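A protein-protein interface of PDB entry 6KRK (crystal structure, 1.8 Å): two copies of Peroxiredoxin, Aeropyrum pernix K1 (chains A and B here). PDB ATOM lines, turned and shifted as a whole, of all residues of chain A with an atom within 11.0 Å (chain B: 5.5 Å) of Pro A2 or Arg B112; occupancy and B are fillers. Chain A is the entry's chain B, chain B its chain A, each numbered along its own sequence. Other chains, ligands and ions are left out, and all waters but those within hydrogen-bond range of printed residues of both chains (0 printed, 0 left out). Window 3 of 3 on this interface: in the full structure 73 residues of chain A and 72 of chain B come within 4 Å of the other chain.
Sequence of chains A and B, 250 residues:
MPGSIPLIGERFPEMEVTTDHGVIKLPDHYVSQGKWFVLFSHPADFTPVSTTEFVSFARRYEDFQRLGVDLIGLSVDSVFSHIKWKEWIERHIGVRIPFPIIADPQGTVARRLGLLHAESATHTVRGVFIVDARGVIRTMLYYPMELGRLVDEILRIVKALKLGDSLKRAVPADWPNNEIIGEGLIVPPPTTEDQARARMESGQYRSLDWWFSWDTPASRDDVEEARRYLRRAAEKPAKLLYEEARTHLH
The backbone NH (N) of Ile B5 is in hydrogen-bond range of the backbone carbonyl oxygen (O) of Gly A3 (2.7 Å).
The backbone nitrogen (N) of Pro A2 sits close to the side-chain carboxylate (OE2) of Glu B10 (2.9 Å).
N of Leu B7 sits at hydrogen-bond distance from OE1 of Glu B10.
A ring nitrogen (NE2) of His A117 is in hydrogen-bond range of the backbone carbonyl oxygen of Gly A114.
Ser B4 touches Pro A2.
O of Ile B5 touches CA of Pro A2 (3.4 Å).
CD1 of Leu B7 touches C of Pro A2, 3.7 Å away.
Pro A2 touches Arg B112 (CG to NH1, 3.9 Å).
CA of Ser B4 touches O of Gly A3, 3.3 Å away.
N of Gly A3 touches CD1 of Leu B7, 3.8 Å away.
Ile B5 touches Ile A5.
Leu A116 touches Leu B7.
His A117 touches Leu B7.
Ala A118 touches Glu B10 (CB to CG, 3.8 Å).
Pro A2 touches just these residues of chain B: Ser B4 (3.6 Å), Ile B5 (3.4 Å), Leu B7 (3.7 Å), Glu B10 (2.9 Å) and Arg B112 (3.9 Å).
Arg B112 touches just one residue of chain A: Pro A2 (3.9 Å).
No residue of chain A comes within 4 Å of Pro B6.
No residue of chain A comes within 4 Å of Val B109.
Printed residues of chain A within 4 Å of Leu B7: Pro A2 (3.7 Å), Gly A3 (3.8 Å), Leu A116 (3.8 Å) and His A117 (3.7 Å).
Of the printed residues of chain B, Ala A118 touches Glu B10 (3.8 Å).
Printed residues of chain A within 4 Å of Ile B5: Pro A2, Gly A3 and Ile A5.
Printed residues of chain B within 4 Å of Leu A116: Leu B7 (3.8 Å).
Of the printed residues of chain A, Glu B10 touches Pro A2 and Ala A118.
Leu A7 touches none of the printed residues of chain B.
Gly B114 touches none of the printed residues of chain A.
The nearest residue of chain B that does not touch Pro A2 is Pro B6 (4.5 Å).
The nearest residue of chain A that does not touch Arg B112 is Gly A3 (7.9 Å).
Of the 15 printed residues of chain A, 6 touch a printed residue of chain B.
Ile A5 touches its own counterpart, Ile B5.
Positions printed for both chains: 4, 5, 7, 110, 111, 113 and 114.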
ATOM      1  N   PRO A   2     -25.744  14.985  12.814  1.00  0.00           N
ATOM      2  CA  PRO A   2     -24.570  15.206  13.674  1.00  0.00           C
ATOM      3  C   PRO A   2     -24.561  16.572  14.388  1.00  0.00           C
ATOM      4  O   PRO A   2     -25.477  17.324  14.229  1.00  0.00           O
ATOM      5  CB  PRO A   2     -23.429  15.064  12.651  1.00  0.00           C
ATOM      6  CG  PRO A   2     -23.864  13.865  11.825  1.00  0.00           C
ATOM      7  CD  PRO A   2     -25.378  13.897  11.884  1.00  0.00           C
ATOM      8  N   GLY A   3     -23.527  16.833  15.189  1.00  0.00           N
ATOM      9  CA  GLY A   3     -23.351  18.082  15.957  1.00  0.00           C
ATOM     10  C   GLY A   3     -21.905  18.260  16.366  1.00  0.00           C
ATOM     11  O   GLY A   3     -21.156  17.290  16.337  1.00  0.00           O
ATOM     12  N   SER A   4     -21.517  19.473  16.722  1.00  0.00           N
ATOM     13  CA  SER A   4     -20.118  19.840  17.027  1.00  0.00           C
ATOM     14  C   SER A   4     -19.849  19.558  18.512  1.00  0.00           C
ATOM     15  O   SER A   4     -20.745  19.811  19.330  1.00  0.00           O
ATOM     16  CB  SER A   4     -19.900  21.282  16.663  1.00  0.00           C
ATOM     17  OG  SER A   4     -18.521  21.597  16.763  1.00  0.00           O
ATOM     18  N   ILE A   5     -18.681  19.046  18.884  1.00  0.00           N
ATOM     19  CA  ILE A   5     -18.275  19.028  20.327  1.00  0.00           C
ATOM     20  C   ILE A   5     -16.877  19.595  20.509  1.00  0.00           C
ATOM     21  O   ILE A   5     -16.044  19.517  19.613  1.00  0.00           O
ATOM     22  CB  ILE A   5     -18.346  17.621  20.934  1.00  0.00           C
ATOM     23  CG1 ILE A   5     -17.567  16.596  20.096  1.00  0.00           C
ATOM     24  CG2 ILE A   5     -19.797  17.217  21.164  1.00  0.00           C
ATOM     25  CD1 ILE A   5     -17.147  15.364  20.879  1.00  0.00           C
ATOM     26  N   LEU A   7     -13.123  19.065  22.083  1.00  0.00           N
ATOM     27  CA  LEU A   7     -12.343  17.816  21.904  1.00  0.00           C
ATOM     28  C   LEU A   7     -11.336  17.640  23.031  1.00  0.00           C
ATOM     29  O   LEU A   7     -10.869  18.613  23.616  1.00  0.00           O
ATOM     30  CB  LEU A   7     -11.640  17.859  20.553  1.00  0.00           C
ATOM     31  CG  LEU A   7     -12.537  18.004  19.336  1.00  0.00           C
ATOM     32  CD1 LEU A   7     -11.667  18.216  18.098  1.00  0.00           C
ATOM     33  CD2 LEU A   7     -13.443  16.804  19.188  1.00  0.00           C
ATOM     34  N   ALA A 110     -25.158  24.613  26.272  1.00  0.00           N
ATOM     35  CA  ALA A 110     -25.445  23.284  25.685  1.00  0.00           C
ATOM     36  C   ALA A 110     -24.918  23.214  24.247  1.00  0.00           C
ATOM     37  O   ALA A 110     -24.306  22.246  23.907  1.00  0.00           O
ATOM     38  CB  ALA A 110     -26.925  22.987  25.749  1.00  0.00           C
ATOM     39  N   ARG A 111     -25.205  24.206  23.406  1.00  0.00           N
ATOM     40  CA  ARG A 111     -24.783  24.184  21.969  1.00  0.00           C
ATOM     41  C   ARG A 111     -23.264  24.235  21.860  1.00  0.00           C
ATOM     42  O   ARG A 111     -22.715  23.451  21.122  1.00  0.00           O
ATOM     43  CB  ARG A 111     -25.476  25.301  21.178  1.00  0.00           C
ATOM     44  CG  ARG A 111     -26.875  24.899  20.740  1.00  0.00           C
ATOM     45  CD  ARG A 111     -27.528  25.962  19.880  1.00  0.00           C
ATOM     46  NE  ARG A 111     -28.423  26.704  20.756  1.00  0.00           N
ATOM     47  CZ  ARG A 111     -28.231  27.937  21.191  1.00  0.00           C
ATOM     48  NH1 ARG A 111     -27.172  28.643  20.820  1.00  0.00           N
ATOM     49  NH2 ARG A 111     -29.122  28.462  22.013  1.00  0.00           N
ATOM     50  N   LEU A 113     -21.125  23.105  23.943  1.00  0.00           N
ATOM     51  CA  LEU A 113     -20.529  21.860  24.461  1.00  0.00           C
ATOM     52  C   LEU A 113     -21.076  20.640  23.710  1.00  0.00           C
ATOM     53  O   LEU A 113     -20.747  19.503  24.117  1.00  0.00           O
ATOM     54  CB  LEU A 113     -20.841  21.769  25.957  1.00  0.00           C
ATOM     55  CG  LEU A 113     -20.170  22.836  26.820  1.00  0.00           C
ATOM     56  CD1 LEU A 113     -20.386  22.509  28.289  1.00  0.00           C
ATOM     57  CD2 LEU A 113     -18.672  22.930  26.502  1.00  0.00           C
ATOM     58  N   GLY A 114     -21.994  20.836  22.769  1.00  0.00           N
ATOM     59  CA  GLY A 114     -22.561  19.715  21.985  1.00  0.00           C
ATOM     60  C   GLY A 114     -23.411  18.750  22.807  1.00  0.00           C
ATOM     61  O   GLY A 114     -23.404  17.566  22.520  1.00  0.00           O
ATOM     62  N   LEU A 115     -24.200  19.267  23.752  1.00  0.00           N
ATOM     63  CA  LEU A 115     -25.006  18.466  24.709  1.00  0.00           C
ATOM     64  C   LEU A 115     -26.458  18.315  24.267  1.00  0.00           C
ATOM     65  O   LEU A 115     -27.204  17.592  24.993  1.00  0.00           O
ATOM     66  CB  LEU A 115     -24.960  19.154  26.063  1.00  0.00           C
ATOM     67  CG  LEU A 115     -23.588  19.138  26.720  1.00  0.00           C
ATOM     68  CD1 LEU A 115     -23.608  20.042  27.924  1.00  0.00           C
ATOM     69  CD2 LEU A 115     -23.216  17.697  27.068  1.00  0.00           C
ATOM     70  N   LEU A 116     -26.837  18.881  23.118  1.00  0.00           N
ATOM     71  CA  LEU A 116     -28.181  18.625  22.534  1.00  0.00           C
ATOM     72  C   LEU A 116     -28.045  17.562  21.459  1.00  0.00           C
ATOM     73  O   LEU A 116     -27.512  17.831  20.362  1.00  0.00           O
ATOM     74  CB  LEU A 116     -28.807  19.907  21.970  1.00  0.00           C
ATOM     75  CG  LEU A 116     -29.045  21.012  22.999  1.00  0.00           C
ATOM     76  CD1 LEU A 116     -29.506  22.285  22.304  1.00  0.00           C
ATOM     77  CD2 LEU A 116     -30.059  20.594  24.059  1.00  0.00           C
ATOM     78  N   HIS A 117     -28.503  16.370  21.755  1.00  0.00           N
ATOM     79  CA  HIS A 117     -28.435  15.216  20.836  1.00  0.00           C
ATOM     80  C   HIS A 117     -29.843  14.957  20.285  1.00  0.00           C
ATOM     81  O   HIS A 117     -30.787  15.735  20.551  1.00  0.00           O
ATOM     82  CB  HIS A 117     -27.823  13.999  21.543  1.00  0.00           C
ATOM     83  CG  HIS A 117     -26.399  14.165  21.924  1.00  0.00           C
ATOM     84  ND1 HIS A 117     -25.508  13.107  21.840  1.00  0.00           N
ATOM     85  CD2 HIS A 117     -25.696  15.254  22.319  1.00  0.00           C
ATOM     86  CE1 HIS A 117     -24.300  13.531  22.186  1.00  0.00           C
ATOM     87  NE2 HIS A 117     -24.387  14.860  22.500  1.00  0.00           N
ATOM     88  N   ALA A 118     -30.005  13.877  19.549  1.00  0.00           N
ATOM     89  CA  ALA A 118     -31.268  13.582  18.827  1.00  0.00           C
ATOM     90  C   ALA A 118     -32.350  13.101  19.791  1.00  0.00           C
ATOM     91  O   ALA A 118     -33.527  13.253  19.456  1.00  0.00           O
ATOM     92  CB  ALA A 118     -30.986  12.584  17.754  1.00  0.00           C
ATOM     93  N   GLU A 119     -32.006  12.598  20.974  1.00  0.00           N
ATOM     94  CA  GLU A 119     -33.025  12.114  21.931  1.00  0.00           C
ATOM     95  C   GLU A 119     -33.934  13.251  22.367  1.00  0.00           C
ATOM     96  O   GLU A 119     -35.052  12.978  22.808  1.00  0.00           O
ATOM     97  CB  GLU A 119     -32.404  11.549  23.213  1.00  0.00           C
ATOM     98  CG  GLU A 119     -32.311  10.065  23.202  1.00  0.00           C
ATOM     99  CD  GLU A 119     -31.960   9.480  24.557  1.00  0.00           C
ATOM    100  OE1 GLU A 119     -32.546   8.432  24.870  1.00  0.00           O
ATOM    101  OE2 GLU A 119     -31.134  10.093  25.306  1.00  0.00           O
ATOM    102  N   SER A 120     -33.426  14.477  22.388  1.00  0.00           N
ATOM    103  CA  SER A 120     -34.246  15.652  22.788  1.00  0.00           C
ATOM    104  C   SER A 120     -33.765  16.917  22.086  1.00  0.00           C
ATOM    105  O   SER A 120     -32.577  17.262  22.155  1.00  0.00           O
ATOM    106  CB  SER A 120     -34.287  15.812  24.268  1.00  0.00           C
ATOM    107  OG  SER A 120     -34.947  17.003  24.619  1.00  0.00           O
ATOM    108  N   SER B   4     -17.011  17.523  14.654  1.00  0.00           N
ATOM    109  CA  SER B   4     -18.405  17.017  14.545  1.00  0.00           C
ATOM    110  C   SER B   4     -18.418  15.583  15.114  1.00  0.00           C
ATOM    111  O   SER B   4     -17.423  14.857  14.928  1.00  0.00           O
ATOM    112  CB  SER B   4     -18.909  17.122  13.104  1.00  0.00           C
ATOM    113  OG  SER B   4     -20.171  16.472  12.927  1.00  0.00           O
ATOM    114  N   ILE B   5     -19.434  15.217  15.892  1.00  0.00           N
ATOM    115  CA  ILE B   5     -19.676  13.784  16.251  1.00  0.00           C
ATOM    116  C   ILE B   5     -21.084  13.362  15.843  1.00  0.00           C
ATOM    117  O   ILE B   5     -21.980  14.186  15.664  1.00  0.00           O
ATOM    118  CB  ILE B   5     -19.428  13.543  17.746  1.00  0.00           C
ATOM    119  CG1 ILE B   5     -20.323  14.429  18.616  1.00  0.00           C
ATOM    120  CG2 ILE B   5     -17.954  13.720  18.072  1.00  0.00           C
ATOM    121  CD1 ILE B   5     -20.458  13.930  20.035  1.00  0.00           C
ATOM    122  N   PRO B   6     -21.326  12.045  15.669  1.00  0.00           N
ATOM    123  CA  PRO B   6     -22.685  11.529  15.565  1.00  0.00           C
ATOM    124  C   PRO B   6     -23.301  11.730  16.958  1.00  0.00           C
ATOM    125  O   PRO B   6     -22.553  12.018  17.890  1.00  0.00           O
ATOM    126  CB  PRO B   6     -22.535  10.033  15.236  1.00  0.00           C
ATOM    127  CG  PRO B   6     -21.061   9.848  14.909  1.00  0.00           C
ATOM    128  CD  PRO B   6     -20.317  10.975  15.598  1.00  0.00           C
ATOM    129  N   LEU B   7     -24.624  11.651  17.063  1.00  0.00           N
ATOM    130  CA  LEU B   7     -25.303  11.984  18.344  1.00  0.00           C
ATOM    131  C   LEU B   7     -26.120  10.814  18.848  1.00  0.00           C
ATOM    132  O   LEU B   7     -26.654  10.021  18.078  1.00  0.00           O
ATOM    133  CB  LEU B   7     -26.169  13.242  18.223  1.00  0.00           C
ATOM    134  CG  LEU B   7     -25.417  14.463  17.691  1.00  0.00           C
ATOM    135  CD1 LEU B   7     -26.366  15.619  17.432  1.00  0.00           C
ATOM    136  CD2 LEU B   7     -24.303  14.894  18.625  1.00  0.00           C
ATOM    137  N   GLU B  10     -29.403   9.138  17.113  1.00  0.00           N
ATOM    138  CA  GLU B  10     -29.241   9.106  15.633  1.00  0.00           C
ATOM    139  C   GLU B  10     -28.917   7.683  15.208  1.00  0.00           C
ATOM    140  O   GLU B  10     -28.258   6.937  15.986  1.00  0.00           O
ATOM    141  CB  GLU B  10     -28.101   9.983  15.138  1.00  0.00           C
ATOM    142  CG  GLU B  10     -28.380  11.469  15.236  1.00  0.00           C
ATOM    143  CD  GLU B  10     -27.271  12.366  14.711  1.00  0.00           C
ATOM    144  OE1 GLU B  10     -26.134  11.891  14.490  1.00  0.00           O
ATOM    145  OE2 GLU B  10     -27.533  13.573  14.589  1.00  0.00           O
ATOM    146  N   PRO B  13     -24.014   6.222  11.340  1.00  0.00           N
ATOM    147  CA  PRO B  13     -23.875   6.606   9.927  1.00  0.00           C
ATOM    148  C   PRO B  13     -23.562   5.388   9.050  1.00  0.00           C
ATOM    149  O   PRO B  13     -22.703   4.591   9.423  1.00  0.00           O
ATOM    150  CB  PRO B  13     -22.715   7.586   9.877  1.00  0.00           C
ATOM    151  CG  PRO B  13     -22.427   7.948  11.314  1.00  0.00           C
ATOM    152  CD  PRO B  13     -23.100   6.926  12.222  1.00  0.00           C
ATOM    153  N   MET B  15     -21.939   3.131   6.536  1.00  0.00           N
ATOM    154  CA  MET B  15     -20.586   3.115   5.932  1.00  0.00           C
ATOM    155  C   MET B  15     -20.165   1.683   5.680  1.00  0.00           C
ATOM    156  O   MET B  15     -20.571   0.763   6.405  1.00  0.00           O
ATOM    157  CB  MET B  15     -19.560   3.791   6.849  1.00  0.00           C
ATOM    158  CG  MET B  15     -19.683   3.301   8.273  1.00  0.00           C
ATOM    159  SD  MET B  15     -18.407   4.006   9.366  1.00  0.00           S
ATOM    160  CE  MET B  15     -19.073   5.650   9.561  1.00  0.00           C
ATOM    161  N   GLY B 107      -8.111   8.028   8.015  1.00  0.00           N
ATOM    162  CA  GLY B 107      -9.045   8.561   9.026  1.00  0.00           C
ATOM    163  C   GLY B 107     -10.392   8.907   8.460  1.00  0.00           C
ATOM    164  O   GLY B 107     -11.032   9.764   9.028  1.00  0.00           O
ATOM    165  N   THR B 108     -10.821   8.265   7.359  1.00  0.00           N
ATOM    166  CA  THR B 108     -12.158   8.461   6.767  1.00  0.00           C
ATOM    167  C   THR B 108     -13.226   8.132   7.808  1.00  0.00           C
ATOM    168  O   THR B 108     -14.151   8.922   7.988  1.00  0.00           O
ATOM    169  CB  THR B 108     -12.364   7.573   5.540  1.00  0.00           C
ATOM    170  OG1 THR B 108     -11.221   7.863   4.732  1.00  0.00           O
ATOM    171  CG2 THR B 108     -13.662   7.869   4.829  1.00  0.00           C
ATOM    172  N   VAL B 109     -13.122   6.972   8.437  1.00  0.00           N
ATOM    173  CA  VAL B 109     -14.111   6.558   9.466  1.00  0.00           C
ATOM    174  C   VAL B 109     -13.907   7.444  10.699  1.00  0.00           C
ATOM    175  O   VAL B 109     -14.892   7.886  11.295  1.00  0.00           O
ATOM    176  CB  VAL B 109     -13.994   5.062   9.814  1.00  0.00           C
ATOM    177  CG1 VAL B 109     -14.934   4.674  10.921  1.00  0.00           C
ATOM    178  CG2 VAL B 109     -14.195   4.165   8.614  1.00  0.00           C
ATOM    179  N   ALA B 110     -12.665   7.666  11.101  1.00  0.00           N
ATOM    180  CA  ALA B 110     -12.353   8.476  12.301  1.00  0.00           C
ATOM    181  C   ALA B 110     -13.025   9.851  12.176  1.00  0.00           C
ATOM    182  O   ALA B 110     -13.673  10.305  13.132  1.00  0.00           O
ATOM    183  CB  ALA B 110     -10.857   8.558  12.453  1.00  0.00           C
ATOM    184  N   ARG B 111     -12.958  10.471  11.006  1.00  0.00           N
ATOM    185  CA  ARG B 111     -13.488  11.850  10.825  1.00  0.00           C
ATOM    186  C   ARG B 111     -15.012  11.795  10.948  1.00  0.00           C
ATOM    187  O   ARG B 111     -15.582  12.619  11.626  1.00  0.00           O
ATOM    188  CB  ARG B 111     -12.997  12.403   9.478  1.00  0.00           C
ATOM    189  CG  ARG B 111     -12.686  13.891   9.476  1.00  0.00           C
ATOM    190  CD  ARG B 111     -11.815  14.277   8.292  1.00  0.00           C
ATOM    191  NE  ARG B 111     -10.532  13.635   8.489  1.00  0.00           N
ATOM    192  CZ  ARG B 111      -9.977  12.715   7.701  1.00  0.00           C
ATOM    193  NH1 ARG B 111     -10.573  12.309   6.586  1.00  0.00           N
ATOM    194  NH2 ARG B 111      -8.789  12.234   8.030  1.00  0.00           N
ATOM    195  N   ARG B 112     -15.650  10.774  10.400  1.00  0.00           N
ATOM    196  CA  ARG B 112     -17.120  10.650  10.415  1.00  0.00           C
ATOM    197  C   ARG B 112     -17.620  10.430  11.852  1.00  0.00           C
ATOM    198  O   ARG B 112     -18.743  10.806  12.120  1.00  0.00           O
ATOM    199  CB  ARG B 112     -17.525   9.544   9.436  1.00  0.00           C
ATOM    200  CG  ARG B 112     -19.017   9.430   9.185  1.00  0.00           C
ATOM    201  CD  ARG B 112     -19.488  10.411   8.135  1.00  0.00           C
ATOM    202  NE  ARG B 112     -20.921  10.347   7.846  1.00  0.00           N
ATOM    203  CZ  ARG B 112     -21.900  10.869   8.602  1.00  0.00           C
ATOM    204  NH1 ARG B 112     -21.634  11.451   9.765  1.00  0.00           N
ATOM    205  NH2 ARG B 112     -23.162  10.772   8.199  1.00  0.00           N
ATOM    206  N   LEU B 113     -16.841   9.779  12.734  1.00  0.00           N
ATOM    207  CA  LEU B 113     -17.249   9.444  14.122  1.00  0.00           C
ATOM    208  C   LEU B 113     -16.683  10.445  15.138  1.00  0.00           C
ATOM    209  O   LEU B 113     -16.877  10.213  16.324  1.00  0.00           O
ATOM    210  CB  LEU B 113     -16.767   8.023  14.435  1.00  0.00           C
ATOM    211  CG  LEU B 113     -17.376   6.963  13.505  1.00  0.00           C
ATOM    212  CD1 LEU B 113     -16.941   5.573  13.916  1.00  0.00           C
ATOM    213  CD2 LEU B 113     -18.903   7.100  13.536  1.00  0.00           C
ATOM    214  N   GLY B 114     -15.935  11.448  14.686  1.00  0.00           N
ATOM    215  CA  GLY B 114     -15.361  12.476  15.575  1.00  0.00           C
ATOM    216  C   GLY B 114     -14.302  11.915  16.493  1.00  0.00           C
ATOM    217  O   GLY B 114     -14.244  12.359  17.671  1.00  0.00           O
